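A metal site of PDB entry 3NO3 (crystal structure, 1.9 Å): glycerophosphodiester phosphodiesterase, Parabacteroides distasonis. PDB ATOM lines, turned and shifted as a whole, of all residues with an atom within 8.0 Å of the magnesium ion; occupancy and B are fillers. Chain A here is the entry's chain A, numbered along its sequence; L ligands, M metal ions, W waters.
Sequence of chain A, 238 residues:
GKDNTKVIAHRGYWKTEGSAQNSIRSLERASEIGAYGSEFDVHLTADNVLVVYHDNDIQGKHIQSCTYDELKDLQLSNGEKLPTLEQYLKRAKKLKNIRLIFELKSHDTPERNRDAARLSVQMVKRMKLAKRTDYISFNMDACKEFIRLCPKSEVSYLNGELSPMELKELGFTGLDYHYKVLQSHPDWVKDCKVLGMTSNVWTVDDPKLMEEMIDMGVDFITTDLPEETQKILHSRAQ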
ATOM      1  N   HIS A  10      27.360 -25.524   3.815  1.00  0.00           N
ATOM      2  CA  HIS A  10      26.428 -26.067   2.840  1.00  0.00           C
ATOM      3  C   HIS A  10      26.915 -27.450   2.393  1.00  0.00           C
ATOM      4  O   HIS A  10      28.050 -27.550   1.887  1.00  0.00           O
ATOM      5  CB  HIS A  10      26.416 -25.145   1.598  1.00  0.00           C
ATOM      6  CG  HIS A  10      25.356 -25.480   0.590  1.00  0.00           C
ATOM      7  ND1 HIS A  10      25.621 -25.682  -0.755  1.00  0.00           N
ATOM      8  CD2 HIS A  10      24.001 -25.546   0.724  1.00  0.00           C
ATOM      9  CE1 HIS A  10      24.475 -25.886  -1.387  1.00  0.00           C
ATOM     10  NE2 HIS A  10      23.481 -25.835  -0.517  1.00  0.00           N
ATOM     11  N   ARG A  11      26.075 -28.485   2.570  1.00  0.00           N
ATOM     12  CA  ARG A  11      26.414 -29.905   2.261  1.00  0.00           C
ATOM     13  C   ARG A  11      27.601 -30.436   3.085  1.00  0.00           C
ATOM     14  O   ARG A  11      28.280 -31.364   2.677  1.00  0.00           O
ATOM     15  CB  ARG A  11      26.622 -30.133   0.755  1.00  0.00           C
ATOM     16  CG  ARG A  11      25.397 -29.658  -0.051  1.00  0.00           C
ATOM     17  CD  ARG A  11      25.530 -29.736  -1.545  1.00  0.00           C
ATOM     18  NE  ARG A  11      24.406 -29.039  -2.169  1.00  0.00           N
ATOM     19  CZ  ARG A  11      24.237 -28.889  -3.493  1.00  0.00           C
ATOM     20  NH1 ARG A  11      25.059 -29.415  -4.385  1.00  0.00           N
ATOM     21  NH2 ARG A  11      23.194 -28.222  -3.935  1.00  0.00           N
ATOM     22  N   ASN A  22      27.519 -33.791   1.186  1.00  0.00           N
ATOM     23  CA  ASN A  22      26.535 -34.658   1.874  1.00  0.00           C
ATOM     24  C   ASN A  22      27.089 -35.996   2.356  1.00  0.00           C
ATOM     25  O   ASN A  22      26.464 -37.049   2.211  1.00  0.00           O
ATOM     26  CB  ASN A  22      25.272 -34.834   0.999  1.00  0.00           C
ATOM     27  CG  ASN A  22      24.345 -33.632   1.023  1.00  0.00           C
ATOM     28  OD1 ASN A  22      24.021 -33.178   2.097  1.00  0.00           O
ATOM     29  ND2 ASN A  22      23.880 -33.146  -0.123  1.00  0.00           N
ATOM     30  N   GLU A  39      24.821 -28.359   6.940  1.00  0.00           N
ATOM     31  CA  GLU A  39      23.601 -28.589   6.164  1.00  0.00           C
ATOM     32  C   GLU A  39      23.715 -29.868   5.343  1.00  0.00           C
ATOM     33  O   GLU A  39      24.816 -30.253   4.873  1.00  0.00           O
ATOM     34  CB  GLU A  39      23.308 -27.372   5.300  1.00  0.00           C
ATOM     35  CG  GLU A  39      21.971 -27.427   4.552  1.00  0.00           C
ATOM     36  CD  GLU A  39      22.044 -27.875   3.103  1.00  0.00           C
ATOM     37  OE1 GLU A  39      23.112 -28.284   2.571  1.00  0.00           O
ATOM     38  OE2 GLU A  39      20.980 -27.736   2.415  1.00  0.00           O
ATOM     39  N   PHE A  40      22.575 -30.541   5.202  1.00  0.00           N
ATOM     40  CA  PHE A  40      22.488 -31.755   4.415  1.00  0.00           C
ATOM     41  C   PHE A  40      21.079 -31.956   3.863  1.00  0.00           C
ATOM     42  O   PHE A  40      20.115 -31.438   4.431  1.00  0.00           O
ATOM     43  CB  PHE A  40      23.012 -32.944   5.263  1.00  0.00           C
ATOM     44  CG  PHE A  40      22.275 -33.131   6.535  1.00  0.00           C
ATOM     45  CD1 PHE A  40      21.154 -33.935   6.589  1.00  0.00           C
ATOM     46  CD2 PHE A  40      22.694 -32.495   7.702  1.00  0.00           C
ATOM     47  CE1 PHE A  40      20.473 -34.086   7.778  1.00  0.00           C
ATOM     48  CE2 PHE A  40      22.004 -32.656   8.888  1.00  0.00           C
ATOM     49  CZ  PHE A  40      20.888 -33.458   8.918  1.00  0.00           C
ATOM     50  N   ASP A  41      20.985 -32.702   2.750  1.00  0.00           N
ATOM     51  CA  ASP A  41      19.753 -32.872   2.010  1.00  0.00           C
ATOM     52  C   ASP A  41      19.201 -34.281   2.158  1.00  0.00           C
ATOM     53  O   ASP A  41      19.926 -35.260   2.028  1.00  0.00           O
ATOM     54  CB  ASP A  41      20.016 -32.573   0.548  1.00  0.00           C
ATOM     55  CG  ASP A  41      20.666 -31.250   0.355  1.00  0.00           C
ATOM     56  OD1 ASP A  41      20.023 -30.236   0.714  1.00  0.00           O
ATOM     57  OD2 ASP A  41      21.791 -31.159  -0.186  1.00  0.00           O
ATOM     58  N   VAL A  42      17.904 -34.383   2.419  1.00  0.00           N
ATOM     59  CA  VAL A  42      17.279 -35.671   2.776  1.00  0.00           C
ATOM     60  C   VAL A  42      16.119 -36.025   1.817  1.00  0.00           C
ATOM     61  O   VAL A  42      15.269 -35.179   1.560  1.00  0.00           O
ATOM     62  CB  VAL A  42      16.807 -35.653   4.211  1.00  0.00           C
ATOM     63  CG1 VAL A  42      16.169 -37.054   4.606  1.00  0.00           C
ATOM     64  CG2 VAL A  42      17.986 -35.254   5.153  1.00  0.00           C
ATOM     65  N   TYR A  53      21.325 -37.065   0.202  1.00  0.00           N
ATOM     66  CA  TYR A  53      21.846 -36.772  -1.151  1.00  0.00           C
ATOM     67  C   TYR A  53      21.148 -35.523  -1.728  1.00  0.00           C
ATOM     68  O   TYR A  53      19.966 -35.308  -1.453  1.00  0.00           O
ATOM     69  CB  TYR A  53      21.644 -37.980  -2.098  1.00  0.00           C
ATOM     70  CG  TYR A  53      22.546 -37.942  -3.318  1.00  0.00           C
ATOM     71  CD1 TYR A  53      23.899 -38.253  -3.228  1.00  0.00           C
ATOM     72  CD2 TYR A  53      22.046 -37.565  -4.558  1.00  0.00           C
ATOM     73  CE1 TYR A  53      24.729 -38.212  -4.313  1.00  0.00           C
ATOM     74  CE2 TYR A  53      22.885 -37.529  -5.697  1.00  0.00           C
ATOM     75  CZ  TYR A  53      24.232 -37.848  -5.550  1.00  0.00           C
ATOM     76  OH  TYR A  53      25.055 -37.805  -6.620  1.00  0.00           O
ATOM     77  N   HIS A  54      21.880 -34.671  -2.468  1.00  0.00           N
ATOM     78  CA  HIS A  54      21.285 -33.441  -2.984  1.00  0.00           C
ATOM     79  C   HIS A  54      20.341 -33.675  -4.167  1.00  0.00           C
ATOM     80  O   HIS A  54      19.169 -33.298  -4.116  1.00  0.00           O
ATOM     81  CB  HIS A  54      22.315 -32.393  -3.398  1.00  0.00           C
ATOM     82  CG  HIS A  54      21.708 -31.292  -4.218  1.00  0.00           C
ATOM     83  ND1 HIS A  54      20.730 -30.436  -3.723  1.00  0.00           N
ATOM     84  CD2 HIS A  54      21.887 -30.939  -5.516  1.00  0.00           C
ATOM     85  CE1 HIS A  54      20.364 -29.601  -4.688  1.00  0.00           C
ATOM     86  NE2 HIS A  54      21.050 -29.882  -5.781  1.00  0.00           N
ATOM     87  N   ILE A 101      21.507 -28.732  10.119  1.00  0.00           N
ATOM     88  CA  ILE A 101      20.615 -27.973   9.257  1.00  0.00           C
ATOM     89  C   ILE A 101      20.063 -28.941   8.205  1.00  0.00           C
ATOM     90  O   ILE A 101      20.711 -29.254   7.227  1.00  0.00           O
ATOM     91  CB  ILE A 101      21.313 -26.737   8.608  1.00  0.00           C
ATOM     92  CG1 ILE A 101      22.054 -25.880   9.666  1.00  0.00           C
ATOM     93  CG2 ILE A 101      20.295 -25.907   7.877  1.00  0.00           C
ATOM     94  CD1 ILE A 101      21.209 -25.361  10.836  1.00  0.00           C
ATOM     95  N   PHE A 102      18.852 -29.441   8.446  1.00  0.00           N
ATOM     96  CA  PHE A 102      18.280 -30.613   7.800  1.00  0.00           C
ATOM     97  C   PHE A 102      17.379 -30.069   6.706  1.00  0.00           C
ATOM     98  O   PHE A 102      16.317 -29.537   7.017  1.00  0.00           O
ATOM     99  CB  PHE A 102      17.478 -31.336   8.897  1.00  0.00           C
ATOM    100  CG  PHE A 102      16.837 -32.677   8.528  1.00  0.00           C
ATOM    101  CD1 PHE A 102      15.916 -32.847   7.479  1.00  0.00           C
ATOM    102  CD2 PHE A 102      17.048 -33.765   9.361  1.00  0.00           C
ATOM    103  CE1 PHE A 102      15.306 -34.056   7.244  1.00  0.00           C
ATOM    104  CE2 PHE A 102      16.451 -34.977   9.132  1.00  0.00           C
ATOM    105  CZ  PHE A 102      15.599 -35.131   8.080  1.00  0.00           C
ATOM    106  N   GLU A 103      17.816 -30.168   5.454  1.00  0.00           N
ATOM    107  CA  GLU A 103      16.947 -29.857   4.328  1.00  0.00           C
ATOM    108  C   GLU A 103      16.133 -31.092   3.922  1.00  0.00           C
ATOM    109  O   GLU A 103      16.717 -32.080   3.431  1.00  0.00           O
ATOM    110  CB  GLU A 103      17.696 -29.299   3.112  1.00  0.00           C
ATOM    111  CG  GLU A 103      16.690 -28.939   2.013  1.00  0.00           C
ATOM    112  CD  GLU A 103      17.278 -28.279   0.766  1.00  0.00           C
ATOM    113  OE1 GLU A 103      18.438 -27.776   0.783  1.00  0.00           O
ATOM    114  OE2 GLU A 103      16.527 -28.194  -0.214  1.00  0.00           O
ATOM    115  N   LEU A 104      14.816 -31.054   4.076  1.00  0.00           N
ATOM    116  CA  LEU A 104      13.991 -32.115   3.460  1.00  0.00           C
ATOM    117  C   LEU A 104      13.733 -31.700   2.002  1.00  0.00           C
ATOM    118  O   LEU A 104      13.143 -30.630   1.730  1.00  0.00           O
ATOM    119  CB  LEU A 104      12.665 -32.349   4.182  1.00  0.00           C
ATOM    120  CG  LEU A 104      11.854 -33.565   3.762  1.00  0.00           C
ATOM    121  CD1 LEU A 104      12.666 -34.923   3.967  1.00  0.00           C
ATOM    122  CD2 LEU A 104      10.463 -33.567   4.515  1.00  0.00           C
ATOM    123  N   LYS A 105      14.142 -32.544   1.078  1.00  0.00           N
ATOM    124  CA  LYS A 105      13.883 -32.334  -0.361  1.00  0.00           C
ATOM    125  C   LYS A 105      12.415 -32.438  -0.661  1.00  0.00           C
ATOM    126  O   LYS A 105      11.660 -33.073   0.098  1.00  0.00           O
ATOM    127  CB  LYS A 105      14.642 -33.360  -1.183  1.00  0.00           C
ATOM    128  CG  LYS A 105      16.171 -33.259  -1.060  1.00  0.00           C
ATOM    129  CD  LYS A 105      16.768 -32.006  -1.725  1.00  0.00           C
ATOM    130  CE  LYS A 105      16.504 -31.904  -3.257  1.00  0.00           C
ATOM    131  NZ  LYS A 105      17.503 -30.980  -3.882  1.00  0.00           N
ATOM    132  N   ILE A 136      14.740 -27.050   7.182  1.00  0.00           N
ATOM    133  CA  ILE A 136      14.562 -26.135   6.064  1.00  0.00           C
ATOM    134  C   ILE A 136      13.958 -26.913   4.895  1.00  0.00           C
ATOM    135  O   ILE A 136      14.234 -28.094   4.750  1.00  0.00           O
ATOM    136  CB  ILE A 136      15.888 -25.431   5.670  1.00  0.00           C
ATOM    137  CG1 ILE A 136      16.946 -26.411   5.115  1.00  0.00           C
ATOM    138  CG2 ILE A 136      16.502 -24.668   6.910  1.00  0.00           C
ATOM    139  CD1 ILE A 136      18.300 -25.710   4.625  1.00  0.00           C
ATOM    140  N   PHE A 138      12.298 -26.268   0.535  1.00  0.00           N
ATOM    141  CA  PHE A 138      11.547 -25.553  -0.506  1.00  0.00           C
ATOM    142  C   PHE A 138      10.071 -25.844  -0.513  1.00  0.00           C
ATOM    143  O   PHE A 138       9.322 -25.086  -1.138  1.00  0.00           O
ATOM    144  CB  PHE A 138      12.086 -25.907  -1.909  1.00  0.00           C
ATOM    145  CG  PHE A 138      13.437 -25.277  -2.210  1.00  0.00           C
ATOM    146  CD1 PHE A 138      13.519 -24.002  -2.744  1.00  0.00           C
ATOM    147  CD2 PHE A 138      14.614 -25.962  -1.955  1.00  0.00           C
ATOM    148  CE1 PHE A 138      14.764 -23.406  -2.992  1.00  0.00           C
ATOM    149  CE2 PHE A 138      15.855 -25.392  -2.238  1.00  0.00           C
ATOM    150  CZ  PHE A 138      15.913 -24.122  -2.743  1.00  0.00           C
ATOM    151  N   LEU A 158      12.716 -22.084   2.223  1.00  0.00           N
ATOM    152  CA  LEU A 158      13.765 -21.846   1.229  1.00  0.00           C
ATOM    153  C   LEU A 158      13.351 -21.109  -0.035  1.00  0.00           C
ATOM    154  O   LEU A 158      14.204 -20.585  -0.734  1.00  0.00           O
ATOM    155  CB  LEU A 158      14.442 -23.170   0.832  1.00  0.00           C
ATOM    156  CG  LEU A 158      15.440 -23.765   1.818  1.00  0.00           C
ATOM    157  CD1 LEU A 158      15.673 -25.241   1.419  1.00  0.00           C
ATOM    158  CD2 LEU A 158      16.773 -22.985   1.843  1.00  0.00           C
ATOM    159  N   ASP A 176      15.346 -18.655   4.831  1.00  0.00           N
ATOM    160  CA  ASP A 176      16.630 -19.135   4.316  1.00  0.00           C
ATOM    161  C   ASP A 176      16.567 -18.974   2.794  1.00  0.00           C
ATOM    162  O   ASP A 176      16.140 -19.866   2.086  1.00  0.00           O
ATOM    163  CB  ASP A 176      16.829 -20.582   4.767  1.00  0.00           C
ATOM    164  CG  ASP A 176      18.174 -21.111   4.466  1.00  0.00           C
ATOM    165  OD1 ASP A 176      19.066 -20.393   3.979  1.00  0.00           O
ATOM    166  OD2 ASP A 176      18.395 -22.268   4.829  1.00  0.00           O
ATOM    167  N   TRP A 202      21.711 -18.221   1.145  1.00  0.00           N
ATOM    168  CA  TRP A 202      22.435 -19.309   0.432  1.00  0.00           C
ATOM    169  C   TRP A 202      22.672 -18.953  -1.051  1.00  0.00           C
ATOM    170  O   TRP A 202      21.983 -18.066  -1.555  1.00  0.00           O
ATOM    171  CB  TRP A 202      21.656 -20.637   0.523  1.00  0.00           C
ATOM    172  CG  TRP A 202      20.243 -20.609  -0.010  1.00  0.00           C
ATOM    173  CD1 TRP A 202      19.120 -20.356   0.695  1.00  0.00           C
ATOM    174  CD2 TRP A 202      19.816 -20.867  -1.360  1.00  0.00           C
ATOM    175  NE1 TRP A 202      18.025 -20.391  -0.113  1.00  0.00           N
ATOM    176  CE2 TRP A 202      18.416 -20.723  -1.382  1.00  0.00           C
ATOM    177  CE3 TRP A 202      20.492 -21.221  -2.549  1.00  0.00           C
ATOM    178  CZ2 TRP A 202      17.651 -20.896  -2.558  1.00  0.00           C
ATOM    179  CZ3 TRP A 202      19.730 -21.408  -3.721  1.00  0.00           C
ATOM    180  CH2 TRP A 202      18.332 -21.233  -3.715  1.00  0.00           C
ATOM    181  N   THR A 203      23.640 -19.567  -1.756  1.00  0.00           N
ATOM    182  CA  THR A 203      24.809 -20.242  -1.230  1.00  0.00           C
ATOM    183  C   THR A 203      25.879 -19.208  -1.535  1.00  0.00           C
ATOM    184  O   THR A 203      26.092 -18.908  -2.694  1.00  0.00           O
ATOM    185  CB  THR A 203      25.004 -21.599  -1.907  1.00  0.00           C
ATOM    186  OG1 THR A 203      23.930 -22.455  -1.492  1.00  0.00           O
ATOM    187  CG2 THR A 203      26.292 -22.267  -1.490  1.00  0.00           C
ATOM    188  N   THR A 222      25.028 -19.468   4.558  1.00  0.00           N
ATOM    189  CA  THR A 222      25.175 -20.843   4.054  1.00  0.00           C
ATOM    190  C   THR A 222      26.126 -20.764   2.888  1.00  0.00           C
ATOM    191  O   THR A 222      25.881 -20.036   1.917  1.00  0.00           O
ATOM    192  CB  THR A 222      23.817 -21.472   3.655  1.00  0.00           C
ATOM    193  OG1 THR A 222      23.010 -21.591   4.821  1.00  0.00           O
ATOM    194  CG2 THR A 222      23.999 -22.883   3.012  1.00  0.00           C
HETATM  195  C1  LIG L   1      19.412 -24.593  -1.077  1.00  0.00           C
HETATM  196  O1  LIG L   1      19.847 -24.986  -2.335  1.00  0.00           O
HETATM  197  C2  LIG L   1      20.467 -24.854  -0.048  1.00  0.00           C
HETATM  198  O2  LIG L   1      20.868 -26.198  -0.099  1.00  0.00           O
HETATM  199  C3  LIG L   1      19.967 -24.452   1.333  1.00  0.00           C
HETATM  200  O3  LIG L   1      20.752 -24.865   2.431  1.00  0.00           O
HETATM  201 MG    MG M   1      20.355 -28.202   0.460  1.00  0.00          MG
HETATM  202  O   HOH W   1      22.415 -28.665   0.008  1.00  0.00           O
HETATM  203  O   HOH W   2      20.034 -28.452  -1.637  1.00  0.00           O
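O of Phe 40 lies within hydrogen-bond range of N of Glu 103, at 2.8 Å.
O of Glu 103 is in hydrogen-bond range of N of Val 42, 2.8 Å away.
NE of Arg 11 lies within salt-bridge range of OD2 of Asp 41.
OD2 of Asp 41 lies within hydrogen-bond range of ND2 of Asn 22 (2.9 Å).
O of Asp 41 sits at hydrogen-bond distance from N of Tyr 53, at 2.9 Å.
The side-chain carboxylate (OE1) of Glu 39 lies within hydrogen-bond range of the backbone NH (N) of Arg 11, 3.0 Å away.
Three residues have an atom within 4 Å of the magnesium ion: Glu 39, Asp 41 and Glu 103.
The nearest printed residue that does not touch the magnesium ion is His 10 (4.04 Å).
The magnesium ion is bound by the side-chain carboxylate of Glu 103, the side-chain carboxylate of Asp 41, the side-chain carboxylate of Glu 39, water W2, an oxygen (O2) of the ligand and water W1.
Water W1 lies within hydrogen-bond range of OD2 of Asp 41 (2.6 Å), OE1 of Glu 39 (2.7 Å), NE of Arg 11 (3.0 Å) and NE2 of His 10 (3.1 Å).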
